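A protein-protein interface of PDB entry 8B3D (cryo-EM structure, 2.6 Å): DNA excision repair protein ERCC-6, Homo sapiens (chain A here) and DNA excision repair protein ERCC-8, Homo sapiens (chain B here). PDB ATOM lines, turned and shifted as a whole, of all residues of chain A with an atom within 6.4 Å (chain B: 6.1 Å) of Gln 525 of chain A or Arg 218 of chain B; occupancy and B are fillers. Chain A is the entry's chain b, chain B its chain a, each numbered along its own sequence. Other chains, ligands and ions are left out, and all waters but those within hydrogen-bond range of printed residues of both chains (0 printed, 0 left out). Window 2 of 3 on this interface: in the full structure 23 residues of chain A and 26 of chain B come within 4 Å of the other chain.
The side-chain amide oxygen of Gln 525 of chain A is in hydrogen-bond range of the guanidinium group of Arg 218 of chain B (2.4 Å). N of Ala 219 of chain B lies within hydrogen-bond range of O of Gln 525 of chain A.
The guanidinium group of Arg 217 of chain B lies within salt-bridge range of the side-chain carboxylate of Asp 215 of chain B. OD2 of Asp 215 of chain B is in salt-bridge range of NH2 of Arg 218 of chain B (2.8 Å). O of Leu 521 of chain A sits at hydrogen-bond distance from N of Ala 526 of chain A, 3.0 Å away.
O of Gln 524 of chain A touches O of Arg 217 of chain B, at 3.6 Å. Arg 218 of chain B touches Gln 524 of chain A. CB of Ala 526 of chain A touches O of Arg 217 of chain B (3.8 Å). NE2 of His 180 of chain B touches CE2 of Phe 693 of chain A (3.4 Å). Val 216 of chain B touches Phe 693 of chain A (O to CZ, 3.96 Å). CE1 of Phe 693 of chain A touches O of Arg 217 of chain B, at 3.5 Å. Phe 693 of chain A touches Arg 218 of chain B. Ala 219 of chain B touches Phe 693 of chain A.
Gln 525 of chain A touches just these residues of chain B: Arg 218 (2.4 Å) and Ala 219 (3.2 Å). Arg 218 of chain B touches three residues of chain A. Printed residues of chain A within 4 Å of Ala 219 of chain B: Gln 525 (3.2 Å) and Phe 693 (3.2 Å). Printed residues of chain B within 4 Å of Gln 524 of chain A: Arg 217 and Arg 218. Of the printed residues of chain B, Phe 693 of chain A touches His 180 (3.4 Å), Val 216 (3.96 Å), Arg 217 (3.5 Å), Arg 218 (3.0 Å) and Ala 219 (3.2 Å). His 522 of chain A touches none of the printed residues of chain B. Pro 668 of chain A touches none of the printed residues of chain B. The nearest printed residue of chain B that does not touch Ala 526 of chain A is Ala 219 of chain B (4.01 Å).
Of the 11 printed residues of chain B, 5 touch a printed residue of chain A. Hydrophobic or aromatic side chains of chain B that line the printed part of chain A: His 180 and Ala 219. Printed residues of chain A that touch a printed residue of chain B: Gln 524, Gln 525, Ala 526 and Phe 693. Hydrophobic or aromatic side chains of chain A that line the printed part of chain B: Ala 526 and Phe 693. Among the printed residues, no Asp or Glu carboxylate lies within 4 Å of a Lys or Arg side-chain nitrogen of the other chain.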
ATOM      1  N   GLU A 520      -4.399 -11.406  -9.731  1.00  0.00           N
ATOM      2  CA  GLU A 520      -4.187 -11.687 -11.148  1.00  0.00           C
ATOM      3  C   GLU A 520      -5.233 -12.666 -11.666  1.00  0.00           C
ATOM      4  O   GLU A 520      -5.752 -12.506 -12.779  1.00  0.00           O
ATOM      5  CB  GLU A 520      -2.776 -12.222 -11.392  1.00  0.00           C
ATOM      6  CG  GLU A 520      -1.660 -11.280 -10.962  1.00  0.00           C
ATOM      7  CD  GLU A 520      -1.327 -10.254 -12.027  1.00  0.00           C
ATOM      8  OE1 GLU A 520      -2.226  -9.475 -12.405  1.00  0.00           O
ATOM      9  OE2 GLU A 520      -0.165 -10.227 -12.487  1.00  0.00           O
ATOM     10  N   LEU A 521      -5.566 -13.680 -10.864  1.00  0.00           N
ATOM     11  CA  LEU A 521      -6.662 -14.571 -11.229  1.00  0.00           C
ATOM     12  C   LEU A 521      -7.970 -13.803 -11.361  1.00  0.00           C
ATOM     13  O   LEU A 521      -8.744 -14.036 -12.295  1.00  0.00           O
ATOM     14  CB  LEU A 521      -6.812 -15.681 -10.192  1.00  0.00           C
ATOM     15  CG  LEU A 521      -5.680 -16.697 -10.082  1.00  0.00           C
ATOM     16  CD1 LEU A 521      -5.891 -17.541  -8.851  1.00  0.00           C
ATOM     17  CD2 LEU A 521      -5.607 -17.570 -11.321  1.00  0.00           C
ATOM     18  N   HIS A 522      -8.235 -12.886 -10.430  1.00  0.00           N
ATOM     19  CA  HIS A 522      -9.466 -12.106 -10.497  1.00  0.00           C
ATOM     20  C   HIS A 522      -9.521 -11.275 -11.770  1.00  0.00           C
ATOM     21  O   HIS A 522     -10.579 -11.151 -12.397  1.00  0.00           O
ATOM     22  CB  HIS A 522      -9.595 -11.205  -9.272  1.00  0.00           C
ATOM     23  CG  HIS A 522     -10.833 -10.367  -9.275  1.00  0.00           C
ATOM     24  ND1 HIS A 522     -12.063 -10.853  -8.892  1.00  0.00           N
ATOM     25  CD2 HIS A 522     -11.033  -9.075  -9.627  1.00  0.00           C
ATOM     26  CE1 HIS A 522     -12.968  -9.897  -9.003  1.00  0.00           C
ATOM     27  NE2 HIS A 522     -12.368  -8.808  -9.447  1.00  0.00           N
ATOM     28  N   CYS A 523      -8.392 -10.684 -12.161  1.00  0.00           N
ATOM     29  CA  CYS A 523      -8.337  -9.962 -13.427  1.00  0.00           C
ATOM     30  C   CYS A 523      -8.625 -10.891 -14.593  1.00  0.00           C
ATOM     31  O   CYS A 523      -9.358 -10.531 -15.520  1.00  0.00           O
ATOM     32  CB  CYS A 523      -6.970  -9.316 -13.606  1.00  0.00           C
ATOM     33  SG  CYS A 523      -6.615  -8.042 -12.419  1.00  0.00           S
ATOM     34  N   GLN A 524      -8.048 -12.088 -14.569  1.00  0.00           N
ATOM     35  CA  GLN A 524      -8.318 -13.075 -15.601  1.00  0.00           C
ATOM     36  C   GLN A 524      -9.710 -13.681 -15.489  1.00  0.00           C
ATOM     37  O   GLN A 524     -10.129 -14.390 -16.408  1.00  0.00           O
ATOM     38  CB  GLN A 524      -7.269 -14.185 -15.541  1.00  0.00           C
ATOM     39  CG  GLN A 524      -5.989 -13.831 -16.260  1.00  0.00           C
ATOM     40  CD  GLN A 524      -4.924 -14.894 -16.115  1.00  0.00           C
ATOM     41  OE1 GLN A 524      -4.889 -15.625 -15.127  1.00  0.00           O
ATOM     42  NE2 GLN A 524      -4.046 -14.986 -17.107  1.00  0.00           N
ATOM     43  N   GLN A 525     -10.434 -13.411 -14.401  1.00  0.00           N
ATOM     44  CA  GLN A 525     -11.736 -14.025 -14.149  1.00  0.00           C
ATOM     45  C   GLN A 525     -11.630 -15.546 -14.209  1.00  0.00           C
ATOM     46  O   GLN A 525     -12.436 -16.223 -14.851  1.00  0.00           O
ATOM     47  CB  GLN A 525     -12.794 -13.503 -15.122  1.00  0.00           C
ATOM     48  CG  GLN A 525     -13.239 -12.083 -14.837  1.00  0.00           C
ATOM     49  CD  GLN A 525     -14.564 -11.749 -15.485  1.00  0.00           C
ATOM     50  OE1 GLN A 525     -14.613 -11.070 -16.510  1.00  0.00           O
ATOM     51  NE2 GLN A 525     -15.651 -12.220 -14.886  1.00  0.00           N
ATOM     52  N   ALA A 526     -10.612 -16.078 -13.544  1.00  0.00           N
ATOM     53  CA  ALA A 526     -10.353 -17.504 -13.465  1.00  0.00           C
ATOM     54  C   ALA A 526     -10.161 -17.912 -12.013  1.00  0.00           C
ATOM     55  O   ALA A 526      -9.813 -17.099 -11.155  1.00  0.00           O
ATOM     56  CB  ALA A 526      -9.116 -17.884 -14.284  1.00  0.00           C
ATOM     57  N   GLY A 527     -10.401 -19.191 -11.745  1.00  0.00           N
ATOM     58  CA  GLY A 527     -10.250 -19.736 -10.417  1.00  0.00           C
ATOM     59  C   GLY A 527      -8.823 -20.174 -10.141  1.00  0.00           C
ATOM     60  O   GLY A 527      -7.938 -20.082 -10.985  1.00  0.00           O
ATOM     61  N   PRO A 668     -17.225 -16.966 -12.011  1.00  0.00           N
ATOM     62  CA  PRO A 668     -15.915 -17.500 -12.409  1.00  0.00           C
ATOM     63  C   PRO A 668     -14.929 -17.578 -11.257  1.00  0.00           C
ATOM     64  O   PRO A 668     -13.978 -18.362 -11.296  1.00  0.00           O
ATOM     65  CB  PRO A 668     -15.438 -16.503 -13.469  1.00  0.00           C
ATOM     66  CG  PRO A 668     -16.124 -15.248 -13.136  1.00  0.00           C
ATOM     67  CD  PRO A 668     -17.455 -15.627 -12.580  1.00  0.00           C
ATOM     68  N   HIS A 669     -15.142 -16.762 -10.224  1.00  0.00           N
ATOM     69  CA  HIS A 669     -14.183 -16.634  -9.129  1.00  0.00           C
ATOM     70  C   HIS A 669     -14.378 -17.788  -8.146  1.00  0.00           C
ATOM     71  O   HIS A 669     -15.060 -17.684  -7.126  1.00  0.00           O
ATOM     72  CB  HIS A 669     -14.338 -15.287  -8.447  1.00  0.00           C
ATOM     73  CG  HIS A 669     -14.391 -14.135  -9.398  1.00  0.00           C
ATOM     74  ND1 HIS A 669     -13.340 -13.802 -10.224  1.00  0.00           N
ATOM     75  CD2 HIS A 669     -15.373 -13.243  -9.661  1.00  0.00           C
ATOM     76  CE1 HIS A 669     -13.671 -12.752 -10.951  1.00  0.00           C
ATOM     77  NE2 HIS A 669     -14.899 -12.392 -10.629  1.00  0.00           N
ATOM     78  N   PHE A 693     -11.731 -24.085 -12.912  1.00  0.00           N
ATOM     79  CA  PHE A 693     -11.605 -23.596 -14.283  1.00  0.00           C
ATOM     80  C   PHE A 693     -12.034 -24.750 -15.177  1.00  0.00           C
ATOM     81  O   PHE A 693     -11.204 -25.568 -15.592  1.00  0.00           O
ATOM     82  CB  PHE A 693     -10.172 -23.181 -14.603  1.00  0.00           C
ATOM     83  CG  PHE A 693     -10.005 -22.607 -15.974  1.00  0.00           C
ATOM     84  CD1 PHE A 693     -10.397 -21.319 -16.249  1.00  0.00           C
ATOM     85  CD2 PHE A 693      -9.589 -23.389 -17.009  1.00  0.00           C
ATOM     86  CE1 PHE A 693     -10.261 -20.792 -17.515  1.00  0.00           C
ATOM     87  CE2 PHE A 693      -9.459 -22.881 -18.284  1.00  0.00           C
ATOM     88  CZ  PHE A 693      -9.804 -21.582 -18.537  1.00  0.00           C
ATOM     89  N   HIS B 180      -7.042 -28.147 -22.961  1.00  0.00           N
ATOM     90  CA  HIS B 180      -7.972 -27.032 -22.830  1.00  0.00           C
ATOM     91  C   HIS B 180      -9.049 -27.103 -23.904  1.00  0.00           C
ATOM     92  O   HIS B 180      -8.750 -27.267 -25.090  1.00  0.00           O
ATOM     93  CB  HIS B 180      -7.205 -25.716 -22.929  1.00  0.00           C
ATOM     94  CG  HIS B 180      -7.936 -24.533 -22.373  1.00  0.00           C
ATOM     95  ND1 HIS B 180      -7.284 -23.400 -21.937  1.00  0.00           N
ATOM     96  CD2 HIS B 180      -9.256 -24.304 -22.180  1.00  0.00           C
ATOM     97  CE1 HIS B 180      -8.171 -22.524 -21.503  1.00  0.00           C
ATOM     98  NE2 HIS B 180      -9.375 -23.048 -21.639  1.00  0.00           N
ATOM     99  N   LEU B 182     -13.264 -25.442 -24.861  1.00  0.00           N
ATOM    100  CA  LEU B 182     -14.332 -24.492 -24.574  1.00  0.00           C
ATOM    101  C   LEU B 182     -15.678 -25.149 -24.850  1.00  0.00           C
ATOM    102  O   LEU B 182     -15.900 -25.680 -25.942  1.00  0.00           O
ATOM    103  CB  LEU B 182     -14.183 -23.227 -25.421  1.00  0.00           C
ATOM    104  CG  LEU B 182     -12.838 -22.500 -25.352  1.00  0.00           C
ATOM    105  CD1 LEU B 182     -12.662 -21.596 -26.553  1.00  0.00           C
ATOM    106  CD2 LEU B 182     -12.732 -21.703 -24.068  1.00  0.00           C
ATOM    107  N   ILE B 201      -9.192 -12.914 -27.420  1.00  0.00           N
ATOM    108  CA  ILE B 201     -10.557 -12.998 -27.926  1.00  0.00           C
ATOM    109  C   ILE B 201     -10.576 -13.916 -29.140  1.00  0.00           C
ATOM    110  O   ILE B 201      -9.847 -13.691 -30.112  1.00  0.00           O
ATOM    111  CB  ILE B 201     -11.104 -11.605 -28.276  1.00  0.00           C
ATOM    112  CG1 ILE B 201     -11.182 -10.722 -27.023  1.00  0.00           C
ATOM    113  CG2 ILE B 201     -12.464 -11.719 -28.951  1.00  0.00           C
ATOM    114  CD1 ILE B 201     -12.163 -11.184 -25.957  1.00  0.00           C
ATOM    115  N   ASP B 215     -13.265 -15.199 -24.264  1.00  0.00           N
ATOM    116  CA  ASP B 215     -12.018 -14.735 -23.672  1.00  0.00           C
ATOM    117  C   ASP B 215     -11.396 -15.994 -23.080  1.00  0.00           C
ATOM    118  O   ASP B 215     -11.818 -16.464 -22.021  1.00  0.00           O
ATOM    119  CB  ASP B 215     -12.269 -13.648 -22.631  1.00  0.00           C
ATOM    120  CG  ASP B 215     -10.987 -13.082 -22.047  1.00  0.00           C
ATOM    121  OD1 ASP B 215     -10.054 -13.854 -21.756  1.00  0.00           O
ATOM    122  OD2 ASP B 215     -10.911 -11.847 -21.880  1.00  0.00           O
ATOM    123  N   VAL B 216     -10.406 -16.552 -23.779  1.00  0.00           N
ATOM    124  CA  VAL B 216      -9.895 -17.872 -23.427  1.00  0.00           C
ATOM    125  C   VAL B 216      -9.270 -17.890 -22.043  1.00  0.00           C
ATOM    126  O   VAL B 216      -9.157 -18.956 -21.431  1.00  0.00           O
ATOM    127  CB  VAL B 216      -8.892 -18.364 -24.491  1.00  0.00           C
ATOM    128  CG1 VAL B 216      -9.548 -18.393 -25.860  1.00  0.00           C
ATOM    129  CG2 VAL B 216      -7.640 -17.501 -24.508  1.00  0.00           C
ATOM    130  N   ARG B 217      -8.852 -16.733 -21.528  1.00  0.00           N
ATOM    131  CA  ARG B 217      -8.389 -16.673 -20.147  1.00  0.00           C
ATOM    132  C   ARG B 217      -9.528 -16.954 -19.178  1.00  0.00           C
ATOM    133  O   ARG B 217      -9.307 -17.462 -18.074  1.00  0.00           O
ATOM    134  CB  ARG B 217      -7.788 -15.301 -19.859  1.00  0.00           C
ATOM    135  CG  ARG B 217      -6.502 -15.021 -20.599  1.00  0.00           C
ATOM    136  CD  ARG B 217      -6.022 -13.603 -20.348  1.00  0.00           C
ATOM    137  NE  ARG B 217      -6.982 -12.608 -20.825  1.00  0.00           N
ATOM    138  CZ  ARG B 217      -6.976 -11.322 -20.485  1.00  0.00           C
ATOM    139  NH1 ARG B 217      -6.056 -10.839 -19.657  1.00  0.00           N
ATOM    140  NH2 ARG B 217      -7.899 -10.509 -20.980  1.00  0.00           N
ATOM    141  N   ARG B 218     -10.752 -16.623 -19.576  1.00  0.00           N
ATOM    142  CA  ARG B 218     -11.892 -16.662 -18.674  1.00  0.00           C
ATOM    143  C   ARG B 218     -12.326 -18.092 -18.386  1.00  0.00           C
ATOM    144  O   ARG B 218     -12.075 -19.014 -19.165  1.00  0.00           O
ATOM    145  CB  ARG B 218     -13.053 -15.873 -19.273  1.00  0.00           C
ATOM    146  CG  ARG B 218     -13.751 -14.983 -18.287  1.00  0.00           C
ATOM    147  CD  ARG B 218     -14.912 -14.236 -18.939  1.00  0.00           C
ATOM    148  NE  ARG B 218     -14.488 -13.217 -19.902  1.00  0.00           N
ATOM    149  CZ  ARG B 218     -13.721 -12.159 -19.638  1.00  0.00           C
ATOM    150  NH1 ARG B 218     -13.299 -11.889 -18.408  1.00  0.00           N
ATOM    151  NH2 ARG B 218     -13.410 -11.326 -20.622  1.00  0.00           N
ATOM    152  N   ALA B 219     -13.002 -18.263 -17.249  1.00  0.00           N
ATOM    153  CA  ALA B 219     -13.480 -19.558 -16.781  1.00  0.00           C
ATOM    154  C   ALA B 219     -14.991 -19.707 -16.924  1.00  0.00           C
ATOM    155  O   ALA B 219     -15.559 -20.705 -16.477  1.00  0.00           O
ATOM    156  CB  ALA B 219     -13.089 -19.766 -15.321  1.00  0.00           C
ATOM    157  N   SER B 220     -15.654 -18.731 -17.552  1.00  0.00           N
ATOM    158  CA  SER B 220     -17.110 -18.659 -17.543  1.00  0.00           C
ATOM    159  C   SER B 220     -17.688 -18.685 -18.950  1.00  0.00           C
ATOM    160  O   SER B 220     -18.629 -17.941 -19.251  1.00  0.00           O
ATOM    161  CB  SER B 220     -17.588 -17.406 -16.812  1.00  0.00           C
ATOM    162  OG  SER B 220     -17.176 -16.235 -17.495  1.00  0.00           O
ATOM    163  N   GLY B 221     -17.146 -19.520 -19.821  1.00  0.00           N
ATOM    164  CA  GLY B 221     -17.731 -19.710 -21.126  1.00  0.00           C
ATOM    165  C   GLY B 221     -17.579 -18.499 -22.027  1.00  0.00           C
ATOM    166  O   GLY B 221     -16.749 -17.609 -21.817  1.00  0.00           O
ATOM    167  N   LEU B 223     -18.070 -15.055 -24.118  1.00  0.00           N
ATOM    168  CA  LEU B 223     -18.420 -13.681 -23.776  1.00  0.00           C
ATOM    169  C   LEU B 223     -19.742 -13.276 -24.411  1.00  0.00           C
ATOM    170  O   LEU B 223     -20.677 -12.866 -23.715  1.00  0.00           O
ATOM    171  CB  LEU B 223     -17.309 -12.731 -24.228  1.00  0.00           C
ATOM    172  CG  LEU B 223     -16.128 -12.393 -23.317  1.00  0.00           C
ATOM    173  CD1 LEU B 223     -15.379 -11.210 -23.902  1.00  0.00           C
ATOM    174  CD2 LEU B 223     -16.584 -12.057 -21.910  1.00  0.00           C
